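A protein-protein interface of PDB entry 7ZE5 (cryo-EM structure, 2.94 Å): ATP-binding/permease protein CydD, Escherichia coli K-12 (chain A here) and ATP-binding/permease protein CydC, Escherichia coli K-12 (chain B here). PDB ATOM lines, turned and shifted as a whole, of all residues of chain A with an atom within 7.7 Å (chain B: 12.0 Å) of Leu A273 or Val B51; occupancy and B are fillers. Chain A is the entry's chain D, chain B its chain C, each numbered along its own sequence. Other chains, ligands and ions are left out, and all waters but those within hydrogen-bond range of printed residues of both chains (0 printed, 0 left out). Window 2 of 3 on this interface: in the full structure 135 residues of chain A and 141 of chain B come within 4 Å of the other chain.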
ATOM      1  N   TYR A 267      13.697 -17.178  22.295  1.00  0.00           N
ATOM      2  CA  TYR A 267      13.464 -17.918  23.530  1.00  0.00           C
ATOM      3  C   TYR A 267      14.610 -18.874  23.829  1.00  0.00           C
ATOM      4  O   TYR A 267      15.063 -18.971  24.974  1.00  0.00           O
ATOM      5  CB  TYR A 267      12.143 -18.682  23.446  1.00  0.00           C
ATOM      6  CG  TYR A 267      12.098 -19.911  24.324  1.00  0.00           C
ATOM      7  CD1 TYR A 267      11.839 -19.806  25.680  1.00  0.00           C
ATOM      8  CD2 TYR A 267      12.315 -21.174  23.795  1.00  0.00           C
ATOM      9  CE1 TYR A 267      11.802 -20.924  26.486  1.00  0.00           C
ATOM     10  CE2 TYR A 267      12.279 -22.296  24.595  1.00  0.00           C
ATOM     11  CZ  TYR A 267      12.023 -22.164  25.939  1.00  0.00           C
ATOM     12  OH  TYR A 267      11.985 -23.281  26.739  1.00  0.00           O
ATOM     13  N   PHE A 268      15.095 -19.589  22.812  1.00  0.00           N
ATOM     14  CA  PHE A 268      16.150 -20.568  23.049  1.00  0.00           C
ATOM     15  C   PHE A 268      17.491 -19.893  23.291  1.00  0.00           C
ATOM     16  O   PHE A 268      18.255 -20.317  24.164  1.00  0.00           O
ATOM     17  CB  PHE A 268      16.238 -21.537  21.874  1.00  0.00           C
ATOM     18  CG  PHE A 268      15.321 -22.710  21.999  1.00  0.00           C
ATOM     19  CD1 PHE A 268      14.148 -22.765  21.274  1.00  0.00           C
ATOM     20  CD2 PHE A 268      15.625 -23.752  22.852  1.00  0.00           C
ATOM     21  CE1 PHE A 268      13.301 -23.839  21.393  1.00  0.00           C
ATOM     22  CE2 PHE A 268      14.781 -24.830  22.974  1.00  0.00           C
ATOM     23  CZ  PHE A 268      13.618 -24.874  22.242  1.00  0.00           C
ATOM     24  N   GLY A 269      17.798 -18.842  22.529  1.00  0.00           N
ATOM     25  CA  GLY A 269      19.042 -18.126  22.754  1.00  0.00           C
ATOM     26  C   GLY A 269      19.118 -17.524  24.143  1.00  0.00           C
ATOM     27  O   GLY A 269      20.167 -17.554  24.788  1.00  0.00           O
ATOM     28  N   PHE A 270      18.005 -16.967  24.622  1.00  0.00           N
ATOM     29  CA  PHE A 270      17.969 -16.445  25.983  1.00  0.00           C
ATOM     30  C   PHE A 270      18.021 -17.574  27.004  1.00  0.00           C
ATOM     31  O   PHE A 270      18.617 -17.420  28.077  1.00  0.00           O
ATOM     32  CB  PHE A 270      16.714 -15.598  26.189  1.00  0.00           C
ATOM     33  CG  PHE A 270      16.804 -14.216  25.606  1.00  0.00           C
ATOM     34  CD1 PHE A 270      17.711 -13.924  24.603  1.00  0.00           C
ATOM     35  CD2 PHE A 270      15.969 -13.211  26.057  1.00  0.00           C
ATOM     36  CE1 PHE A 270      17.786 -12.657  24.066  1.00  0.00           C
ATOM     37  CE2 PHE A 270      16.040 -11.942  25.525  1.00  0.00           C
ATOM     38  CZ  PHE A 270      16.950 -11.664  24.528  1.00  0.00           C
ATOM     39  N   SER A 271      17.398 -18.711  26.691  1.00  0.00           N
ATOM     40  CA  SER A 271      17.357 -19.822  27.636  1.00  0.00           C
ATOM     41  C   SER A 271      18.739 -20.423  27.852  1.00  0.00           C
ATOM     42  O   SER A 271      19.075 -20.830  28.970  1.00  0.00           O
ATOM     43  CB  SER A 271      16.381 -20.890  27.145  1.00  0.00           C
ATOM     44  OG  SER A 271      16.068 -21.802  28.181  1.00  0.00           O
ATOM     45  N   TYR A 272      19.551 -20.497  26.795  1.00  0.00           N
ATOM     46  CA  TYR A 272      20.891 -21.058  26.937  1.00  0.00           C
ATOM     47  C   TYR A 272      21.764 -20.181  27.825  1.00  0.00           C
ATOM     48  O   TYR A 272      22.583 -20.689  28.599  1.00  0.00           O
ATOM     49  CB  TYR A 272      21.534 -21.241  25.564  1.00  0.00           C
ATOM     50  CG  TYR A 272      20.903 -22.332  24.734  1.00  0.00           C
ATOM     51  CD1 TYR A 272      20.638 -23.578  25.276  1.00  0.00           C
ATOM     52  CD2 TYR A 272      20.579 -22.118  23.404  1.00  0.00           C
ATOM     53  CE1 TYR A 272      20.063 -24.575  24.521  1.00  0.00           C
ATOM     54  CE2 TYR A 272      20.003 -23.109  22.643  1.00  0.00           C
ATOM     55  CZ  TYR A 272      19.746 -24.335  23.204  1.00  0.00           C
ATOM     56  OH  TYR A 272      19.172 -25.325  22.444  1.00  0.00           O
ATOM     57  N   LEU A 273      21.610 -18.861  27.722  1.00  0.00           N
ATOM     58  CA  LEU A 273      22.366 -17.936  28.556  1.00  0.00           C
ATOM     59  C   LEU A 273      21.849 -17.863  29.984  1.00  0.00           C
ATOM     60  O   LEU A 273      22.549 -17.330  30.849  1.00  0.00           O
ATOM     61  CB  LEU A 273      22.337 -16.532  27.951  1.00  0.00           C
ATOM     62  CG  LEU A 273      22.860 -16.365  26.529  1.00  0.00           C
ATOM     63  CD1 LEU A 273      22.640 -14.944  26.056  1.00  0.00           C
ATOM     64  CD2 LEU A 273      24.328 -16.739  26.446  1.00  0.00           C
ATOM     65  N   GLY A 274      20.656 -18.383  30.253  1.00  0.00           N
ATOM     66  CA  GLY A 274      20.051 -18.221  31.555  1.00  0.00           C
ATOM     67  C   GLY A 274      19.279 -16.936  31.739  1.00  0.00           C
ATOM     68  O   GLY A 274      18.864 -16.640  32.865  1.00  0.00           O
ATOM     69  N   GLU A 275      19.080 -16.158  30.671  1.00  0.00           N
ATOM     70  CA  GLU A 275      18.300 -14.929  30.781  1.00  0.00           C
ATOM     71  C   GLU A 275      16.877 -15.222  31.234  1.00  0.00           C
ATOM     72  O   GLU A 275      16.343 -14.540  32.116  1.00  0.00           O
ATOM     73  CB  GLU A 275      18.295 -14.192  29.444  1.00  0.00           C
ATOM     74  CG  GLU A 275      17.714 -12.793  29.507  1.00  0.00           C
ATOM     75  CD  GLU A 275      18.762 -11.740  29.799  1.00  0.00           C
ATOM     76  OE1 GLU A 275      18.463 -10.539  29.634  1.00  0.00           O
ATOM     77  OE2 GLU A 275      19.887 -12.113  30.190  1.00  0.00           O
ATOM     78  N   LEU A 276      16.247 -16.229  30.637  1.00  0.00           N
ATOM     79  CA  LEU A 276      14.948 -16.715  31.080  1.00  0.00           C
ATOM     80  C   LEU A 276      15.002 -18.233  31.106  1.00  0.00           C
ATOM     81  O   LEU A 276      15.549 -18.851  30.189  1.00  0.00           O
ATOM     82  CB  LEU A 276      13.819 -16.210  30.168  1.00  0.00           C
ATOM     83  CG  LEU A 276      13.854 -16.484  28.661  1.00  0.00           C
ATOM     84  CD1 LEU A 276      13.207 -17.813  28.309  1.00  0.00           C
ATOM     85  CD2 LEU A 276      13.184 -15.348  27.907  1.00  0.00           C
ATOM     86  N   ASP A 277      14.454 -18.830  32.160  1.00  0.00           N
ATOM     87  CA  ASP A 277      14.548 -20.273  32.382  1.00  0.00           C
ATOM     88  C   ASP A 277      13.185 -20.855  32.757  1.00  0.00           C
ATOM     89  O   ASP A 277      12.830 -20.951  33.934  1.00  0.00           O
ATOM     90  CB  ASP A 277      15.624 -20.582  33.425  1.00  0.00           C
ATOM     91  CG  ASP A 277      15.376 -19.903  34.766  1.00  0.00           C
ATOM     92  OD1 ASP A 277      14.407 -19.125  34.889  1.00  0.00           O
ATOM     93  OD2 ASP A 277      16.160 -20.153  35.705  1.00  0.00           O
ATOM     94  N   LEU B  38      20.744 -16.400  10.940  1.00  0.00           N
ATOM     95  CA  LEU B  38      20.999 -15.763  12.227  1.00  0.00           C
ATOM     96  C   LEU B  38      20.497 -16.626  13.375  1.00  0.00           C
ATOM     97  O   LEU B  38      21.191 -16.792  14.383  1.00  0.00           O
ATOM     98  CB  LEU B  38      20.344 -14.383  12.276  1.00  0.00           C
ATOM     99  CG  LEU B  38      20.697 -13.496  13.467  1.00  0.00           C
ATOM    100  CD1 LEU B  38      22.185 -13.548  13.754  1.00  0.00           C
ATOM    101  CD2 LEU B  38      20.249 -12.070  13.214  1.00  0.00           C
ATOM    102  N   SER B  39      19.294 -17.188  13.237  1.00  0.00           N
ATOM    103  CA  SER B  39      18.750 -18.043  14.286  1.00  0.00           C
ATOM    104  C   SER B  39      19.620 -19.273  14.501  1.00  0.00           C
ATOM    105  O   SER B  39      19.855 -19.683  15.642  1.00  0.00           O
ATOM    106  CB  SER B  39      17.321 -18.452  13.939  1.00  0.00           C
ATOM    107  OG  SER B  39      16.533 -17.323  13.615  1.00  0.00           O
ATOM    108  N   TRP B  41      22.877 -19.604  13.967  1.00  0.00           N
ATOM    109  CA  TRP B  41      24.095 -19.223  14.671  1.00  0.00           C
ATOM    110  C   TRP B  41      23.789 -18.745  16.083  1.00  0.00           C
ATOM    111  O   TRP B  41      24.521 -19.071  17.024  1.00  0.00           O
ATOM    112  CB  TRP B  41      24.842 -18.140  13.897  1.00  0.00           C
ATOM    113  CG  TRP B  41      25.955 -17.530  14.685  1.00  0.00           C
ATOM    114  CD1 TRP B  41      27.233 -17.988  14.786  1.00  0.00           C
ATOM    115  CD2 TRP B  41      25.887 -16.349  15.492  1.00  0.00           C
ATOM    116  NE1 TRP B  41      27.966 -17.167  15.604  1.00  0.00           N
ATOM    117  CE2 TRP B  41      27.162 -16.154  16.051  1.00  0.00           C
ATOM    118  CE3 TRP B  41      24.869 -15.441  15.796  1.00  0.00           C
ATOM    119  CZ2 TRP B  41      27.449 -15.086  16.896  1.00  0.00           C
ATOM    120  CZ3 TRP B  41      25.156 -14.383  16.634  1.00  0.00           C
ATOM    121  CH2 TRP B  41      26.434 -14.214  17.175  1.00  0.00           C
ATOM    122  N   PHE B  42      22.715 -17.970  16.251  1.00  0.00           N
ATOM    123  CA  PHE B  42      22.397 -17.417  17.564  1.00  0.00           C
ATOM    124  C   PHE B  42      22.152 -18.522  18.581  1.00  0.00           C
ATOM    125  O   PHE B  42      22.636 -18.446  19.715  1.00  0.00           O
ATOM    126  CB  PHE B  42      21.180 -16.498  17.461  1.00  0.00           C
ATOM    127  CG  PHE B  42      20.783 -15.861  18.761  1.00  0.00           C
ATOM    128  CD1 PHE B  42      21.740 -15.473  19.680  1.00  0.00           C
ATOM    129  CD2 PHE B  42      19.451 -15.637  19.056  1.00  0.00           C
ATOM    130  CE1 PHE B  42      21.374 -14.885  20.872  1.00  0.00           C
ATOM    131  CE2 PHE B  42      19.079 -15.049  20.245  1.00  0.00           C
ATOM    132  CZ  PHE B  42      20.042 -14.673  21.154  1.00  0.00           C
ATOM    133  N   LEU B  43      21.414 -19.562  18.194  1.00  0.00           N
ATOM    134  CA  LEU B  43      21.169 -20.676  19.104  1.00  0.00           C
ATOM    135  C   LEU B  43      22.466 -21.394  19.455  1.00  0.00           C
ATOM    136  O   LEU B  43      22.745 -21.658  20.629  1.00  0.00           O
ATOM    137  CB  LEU B  43      20.169 -21.649  18.485  1.00  0.00           C
ATOM    138  CG  LEU B  43      18.732 -21.531  18.985  1.00  0.00           C
ATOM    139  CD1 LEU B  43      18.182 -20.157  18.669  1.00  0.00           C
ATOM    140  CD2 LEU B  43      17.866 -22.610  18.370  1.00  0.00           C
ATOM    141  N   SER B  44      23.272 -21.722  18.443  1.00  0.00           N
ATOM    142  CA  SER B  44      24.513 -22.445  18.695  1.00  0.00           C
ATOM    143  C   SER B  44      25.511 -21.590  19.467  1.00  0.00           C
ATOM    144  O   SER B  44      26.190 -22.088  20.372  1.00  0.00           O
ATOM    145  CB  SER B  44      25.116 -22.920  17.376  1.00  0.00           C
ATOM    146  OG  SER B  44      25.364 -21.829  16.510  1.00  0.00           O
ATOM    147  N   ALA B  45      25.619 -20.303  19.125  1.00  0.00           N
ATOM    148  CA  ALA B  45      26.534 -19.427  19.850  1.00  0.00           C
ATOM    149  C   ALA B  45      26.073 -19.212  21.284  1.00  0.00           C
ATOM    150  O   ALA B  45      26.898 -19.136  22.201  1.00  0.00           O
ATOM    151  CB  ALA B  45      26.670 -18.089  19.128  1.00  0.00           C
ATOM    152  N   SER B  46      24.761 -19.096  21.495  1.00  0.00           N
ATOM    153  CA  SER B  46      24.240 -18.942  22.849  1.00  0.00           C
ATOM    154  C   SER B  46      24.520 -20.179  23.692  1.00  0.00           C
ATOM    155  O   SER B  46      24.912 -20.068  24.858  1.00  0.00           O
ATOM    156  CB  SER B  46      22.743 -18.655  22.801  1.00  0.00           C
ATOM    157  OG  SER B  46      22.289 -18.103  24.018  1.00  0.00           O
ATOM    158  N   ALA B  47      24.320 -21.366  23.119  1.00  0.00           N
ATOM    159  CA  ALA B  47      24.553 -22.597  23.866  1.00  0.00           C
ATOM    160  C   ALA B  47      26.029 -22.776  24.196  1.00  0.00           C
ATOM    161  O   ALA B  47      26.374 -23.209  25.301  1.00  0.00           O
ATOM    162  CB  ALA B  47      24.033 -23.797  23.079  1.00  0.00           C
ATOM    163  N   VAL B  48      26.911 -22.459  23.248  1.00  0.00           N
ATOM    164  CA  VAL B  48      28.345 -22.593  23.489  1.00  0.00           C
ATOM    165  C   VAL B  48      28.784 -21.654  24.605  1.00  0.00           C
ATOM    166  O   VAL B  48      29.565 -22.035  25.487  1.00  0.00           O
ATOM    167  CB  VAL B  48      29.130 -22.342  22.188  1.00  0.00           C
ATOM    168  CG1 VAL B  48      30.577 -21.998  22.493  1.00  0.00           C
ATOM    169  CG2 VAL B  48      29.049 -23.559  21.285  1.00  0.00           C
ATOM    170  N   ALA B  49      28.285 -20.416  24.590  1.00  0.00           N
ATOM    171  CA  ALA B  49      28.615 -19.474  25.654  1.00  0.00           C
ATOM    172  C   ALA B  49      28.115 -19.972  27.004  1.00  0.00           C
ATOM    173  O   ALA B  49      28.817 -19.858  28.014  1.00  0.00           O
ATOM    174  CB  ALA B  49      28.031 -18.099  25.338  1.00  0.00           C
ATOM    175  N   GLY B  50      26.909 -20.527  27.039  1.00  0.00           N
ATOM    176  CA  GLY B  50      26.382 -21.079  28.267  1.00  0.00           C
ATOM    177  C   GLY B  50      25.964 -20.008  29.261  1.00  0.00           C
ATOM    178  O   GLY B  50      25.827 -18.827  28.943  1.00  0.00           O
ATOM    179  N   VAL B  51      25.758 -20.461  30.498  1.00  0.00           N
ATOM    180  CA  VAL B  51      25.348 -19.555  31.568  1.00  0.00           C
ATOM    181  C   VAL B  51      26.430 -18.516  31.831  1.00  0.00           C
ATOM    182  O   VAL B  51      26.141 -17.325  32.003  1.00  0.00           O
ATOM    183  CB  VAL B  51      25.003 -20.353  32.840  1.00  0.00           C
ATOM    184  CG1 VAL B  51      24.872 -19.425  34.037  1.00  0.00           C
ATOM    185  CG2 VAL B  51      23.728 -21.152  32.635  1.00  0.00           C
ATOM    186  N   ALA B  52      27.693 -18.947  31.858  1.00  0.00           N
ATOM    187  CA  ALA B  52      28.794 -18.030  32.128  1.00  0.00           C
ATOM    188  C   ALA B  52      28.944 -16.963  31.052  1.00  0.00           C
ATOM    189  O   ALA B  52      29.605 -15.947  31.290  1.00  0.00           O
ATOM    190  CB  ALA B  52      30.102 -18.809  32.270  1.00  0.00           C
ATOM    191  N   GLY B  53      28.349 -17.168  29.875  1.00  0.00           N
ATOM    192  CA  GLY B  53      28.441 -16.182  28.815  1.00  0.00           C
ATOM    193  C   GLY B  53      27.626 -14.931  29.062  1.00  0.00           C
ATOM    194  O   GLY B  53      27.905 -13.893  28.451  1.00  0.00           O
ATOM    195  N   LEU B  54      26.630 -15.002  29.941  1.00  0.00           N
ATOM    196  CA  LEU B  54      25.806 -13.839  30.231  1.00  0.00           C
ATOM    197  C   LEU B  54      26.647 -12.765  30.915  1.00  0.00           C
ATOM    198  O   LEU B  54      27.650 -13.060  31.572  1.00  0.00           O
ATOM    199  CB  LEU B  54      24.613 -14.243  31.102  1.00  0.00           C
ATOM    200  CG  LEU B  54      23.396 -13.317  31.188  1.00  0.00           C
ATOM    201  CD1 LEU B  54      22.141 -14.141  31.415  1.00  0.00           C
ATOM    202  CD2 LEU B  54      23.538 -12.295  32.294  1.00  0.00           C
ATOM    203  N   TYR B  55      26.245 -11.505  30.714  1.00  0.00           N
ATOM    204  CA  TYR B  55      26.974 -10.310  31.143  1.00  0.00           C
ATOM    205  C   TYR B  55      28.218 -10.100  30.288  1.00  0.00           C
ATOM    206  O   TYR B  55      28.928  -9.102  30.451  1.00  0.00           O
ATOM    207  CB  TYR B  55      27.362 -10.370  32.626  1.00  0.00           C
ATOM    208  CG  TYR B  55      26.197 -10.419  33.589  1.00  0.00           C
ATOM    209  CD1 TYR B  55      26.107 -11.419  34.548  1.00  0.00           C
ATOM    210  CD2 TYR B  55      25.196  -9.457  33.548  1.00  0.00           C
ATOM    211  CE1 TYR B  55      25.047 -11.466  35.434  1.00  0.00           C
ATOM    212  CE2 TYR B  55      24.132  -9.497  34.430  1.00  0.00           C
ATOM    213  CZ  TYR B  55      24.063 -10.503  35.370  1.00  0.00           C
ATOM    214  OH  TYR B  55      23.006 -10.547  36.251  1.00  0.00           O
ATOM    215  N   SER B  56      28.489 -11.031  29.372  1.00  0.00           N
ATOM    216  CA  SER B  56      29.633 -10.929  28.479  1.00  0.00           C
ATOM    217  C   SER B  56      29.305 -11.242  27.028  1.00  0.00           C
ATOM    218  O   SER B  56      30.163 -11.027  26.165  1.00  0.00           O
ATOM    219  CB  SER B  56      30.763 -11.863  28.942  1.00  0.00           C
ATOM    220  OG  SER B  56      31.875 -11.785  28.068  1.00  0.00           O
ATOM    221  N   PHE B  57      28.108 -11.738  26.732  1.00  0.00           N
ATOM    222  CA  PHE B  57      27.688 -12.051  25.373  1.00  0.00           C
ATOM    223  C   PHE B  57      26.586 -11.084  24.966  1.00  0.00           C
ATOM    224  O   PHE B  57      25.556 -10.991  25.642  1.00  0.00           O
ATOM    225  CB  PHE B  57      27.201 -13.500  25.279  1.00  0.00           C
ATOM    226  CG  PHE B  57      26.629 -13.870  23.941  1.00  0.00           C
ATOM    227  CD1 PHE B  57      27.448 -14.349  22.934  1.00  0.00           C
ATOM    228  CD2 PHE B  57      25.270 -13.766  23.696  1.00  0.00           C
ATOM    229  CE1 PHE B  57      26.926 -14.697  21.705  1.00  0.00           C
ATOM    230  CE2 PHE B  57      24.744 -14.112  22.469  1.00  0.00           C
ATOM    231  CZ  PHE B  57      25.573 -14.580  21.473  1.00  0.00           C
ATOM    232  N   ASN B  58      26.803 -10.369  23.865  1.00  0.00           N
ATOM    233  CA  ASN B  58      25.849  -9.369  23.394  1.00  0.00           C
ATOM    234  C   ASN B  58      24.690 -10.087  22.718  1.00  0.00           C
ATOM    235  O   ASN B  58      24.717 -10.343  21.513  1.00  0.00           O
ATOM    236  CB  ASN B  58      26.522  -8.387  22.442  1.00  0.00           C
ATOM    237  CG  ASN B  58      25.618  -7.232  22.064  1.00  0.00           C
ATOM    238  OD1 ASN B  58      24.592  -7.001  22.700  1.00  0.00           O
ATOM    239  ND2 ASN B  58      25.996  -6.502  21.022  1.00  0.00           N
ATOM    240  N   TYR B  59      23.665 -10.417  23.498  1.00  0.00           N
ATOM    241  CA  TYR B  59      22.496 -11.118  22.988  1.00  0.00           C
ATOM    242  C   TYR B  59      21.406 -10.186  22.482  1.00  0.00           C
ATOM    243  O   TYR B  59      20.450 -10.660  21.857  1.00  0.00           O
ATOM    244  CB  TYR B  59      21.922 -12.034  24.074  1.00  0.00           C
ATOM    245  CG  TYR B  59      21.536 -11.310  25.346  1.00  0.00           C
ATOM    246  CD1 TYR B  59      22.428 -11.206  26.404  1.00  0.00           C
ATOM    247  CD2 TYR B  59      20.279 -10.740  25.493  1.00  0.00           C
ATOM    248  CE1 TYR B  59      22.083 -10.547  27.567  1.00  0.00           C
ATOM    249  CE2 TYR B  59      19.925 -10.080  26.653  1.00  0.00           C
ATOM    250  CZ  TYR B  59      20.830  -9.987  27.686  1.00  0.00           C
ATOM    251  OH  TYR B  59      20.480  -9.330  28.843  1.00  0.00           O
ATOM    252  N   MET B  60      21.515  -8.880  22.732  1.00  0.00           N
ATOM    253  CA  MET B  60      20.469  -7.961  22.297  1.00  0.00           C
ATOM    254  C   MET B  60      20.552  -7.688  20.801  1.00  0.00           C
ATOM    255  O   MET B  60      19.523  -7.500  20.143  1.00  0.00           O
ATOM    256  CB  MET B  60      20.549  -6.657  23.088  1.00  0.00           C
ATOM    257  CG  MET B  60      20.248  -6.816  24.566  1.00  0.00           C
ATOM    258  SD  MET B  60      18.580  -7.432  24.862  1.00  0.00           S
ATOM    259  CE  MET B  60      17.599  -6.025  24.352  1.00  0.00           C
ATOM    260  N   LEU B  61      21.764  -7.648  20.250  1.00  0.00           N
ATOM    261  CA  LEU B  61      21.910  -7.397  18.817  1.00  0.00           C
ATOM    262  C   LEU B  61      21.278  -8.487  17.961  1.00  0.00           C
ATOM    263  O   LEU B  61      20.516  -8.148  17.040  1.00  0.00           O
ATOM    264  CB  LEU B  61      23.391  -7.192  18.477  1.00  0.00           C
ATOM    265  CG  LEU B  61      23.718  -6.966  17.002  1.00  0.00           C
ATOM    266  CD1 LEU B  61      23.040  -5.706  16.495  1.00  0.00           C
ATOM    267  CD2 LEU B  61      25.220  -6.889  16.795  1.00  0.00           C
ATOM    268  N   PRO B  62      21.538  -9.784  18.180  1.00  0.00           N
ATOM    269  CA  PRO B  62      20.801 -10.795  17.406  1.00  0.00           C
ATOM    270  C   PRO B  62      19.307 -10.772  17.656  1.00  0.00           C
ATOM    271  O   PRO B  62      18.529 -11.079  16.744  1.00  0.00           O
ATOM    272  CB  PRO B  62      21.433 -12.117  17.865  1.00  0.00           C
ATOM    273  CG  PRO B  62      22.764 -11.738  18.394  1.00  0.00           C
ATOM    274  CD  PRO B  62      22.548 -10.413  19.047  1.00  0.00           C
ATOM    275  N   ALA B  63      18.877 -10.418  18.870  1.00  0.00           N
ATOM    276  CA  ALA B  63      17.449 -10.383  19.169  1.00  0.00           C
ATOM    277  C   ALA B  63      16.732  -9.344  18.319  1.00  0.00           C
ATOM    278  O   ALA B  63      15.593  -9.559  17.891  1.00  0.00           O
ATOM    279  CB  ALA B  63      17.230 -10.106  20.655  1.00  0.00           C
ATOM    280  N   ALA B  64      17.376  -8.202  18.073  1.00  0.00           N
ATOM    281  CA  ALA B  64      16.813  -7.221  17.155  1.00  0.00           C
ATOM    282  C   ALA B  64      16.993  -7.637  15.703  1.00  0.00           C
ATOM    283  O   ALA B  64      16.224  -7.203  14.838  1.00  0.00           O
ATOM    284  CB  ALA B  64      17.448  -5.851  17.391  1.00  0.00           C
ATOM    285  N   ALA B 278      30.014 -22.659  16.996  1.00  0.00           N
ATOM    286  CA  ALA B 278      28.783 -22.103  16.451  1.00  0.00           C
ATOM    287  C   ALA B 278      28.837 -21.912  14.941  1.00  0.00           C
ATOM    288  O   ALA B 278      27.782 -21.850  14.303  1.00  0.00           O
ATOM    289  CB  ALA B 278      28.470 -20.767  17.122  1.00  0.00           C
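The side-chain hydroxyl (OH) of Tyr B59 lies within hydrogen-bond range of the side-chain carboxylate (OE1) of Glu A275, at 2.5 Å. The backbone carbonyl oxygen of Gly A269 sits close to the side-chain hydroxyl of Ser B46 (2.3 Å).
The backbone NH of Glu A275 sits at hydrogen-bond distance from the backbone carbonyl oxygen of Phe A270 (2.9 Å).
Phe A268 touches Leu B43 (CB to CG, 3.8 Å). Tyr A272 touches Leu B43 (CD2 to O, 3.6 Å). OG of Ser B46 touches CB of Tyr A272, at 3.6 Å. Tyr A272 touches Ala B47. Leu A273 touches Ser B46. Val B51 touches Leu A273 (CA to O, 3.6 Å). Leu B54 touches Leu A273 (CD1 to O, 3.3 Å). Phe B57 touches Leu A273. Tyr B59 touches Leu A273 (CB to CD1, 3.6 Å). Glu A275 touches Leu B54.
Leu A273 touches just these residues of chain B: Ser B46 (3.1 Å), Gly B50 (3.6 Å), Val B51 (3.6 Å), Leu B54 (3.3 Å), Phe B57 (3.7 Å) and Tyr B59 (3.6 Å). Val B51 touches just these residues of chain A: Tyr A272 (3.7 Å) and Leu A273 (3.6 Å). Gly A269 touches just these residues of chain B: Phe B42 (3.9 Å) and Ser B46 (2.3 Å). Of the printed residues of chain B, Phe A270 touches Tyr B59 (3.5 Å). Ser A271 touches none of the printed residues of chain B. Glu A275 touches two residues of chain B. Of the printed residues of chain A, Gly B50 touches Tyr A272 and Leu A273. Printed residues of chain B within 4 Å of Phe A268: Leu B43. Printed residues of chain A within 4 Å of Ser B46: Gly A269, Tyr A272 and Leu A273. Of the printed residues of chain B, Tyr A272 touches Leu B43 (3.6 Å), Ser B46 (3.6 Å), Ala B47 (3.7 Å), Gly B50 (3.5 Å) and Val B51 (3.7 Å). Of the printed residues of chain A, Tyr B59 touches Phe A270 (3.5 Å), Leu A273 (3.6 Å) and Glu A275 (2.5 Å). Asn B58 touches none of the printed residues of chain A. The nearest residue of chain A that does not touch Val B51 is Gly A274 (4.8 Å).
Hydrophobic or aromatic side chains of chain A within 4 Å of the printed part of chain B: Phe A268, Phe A270, Tyr A272 and Leu A273. Of the 27 printed residues of chain B, 9 touch a printed residue of chain A. Among the printed residues, 17 pairs touch across the chains. Among the printed residues, no Asp or Glu carboxylate lies within 4 Å of a Lys or Arg side-chain nitrogen of the other chain.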
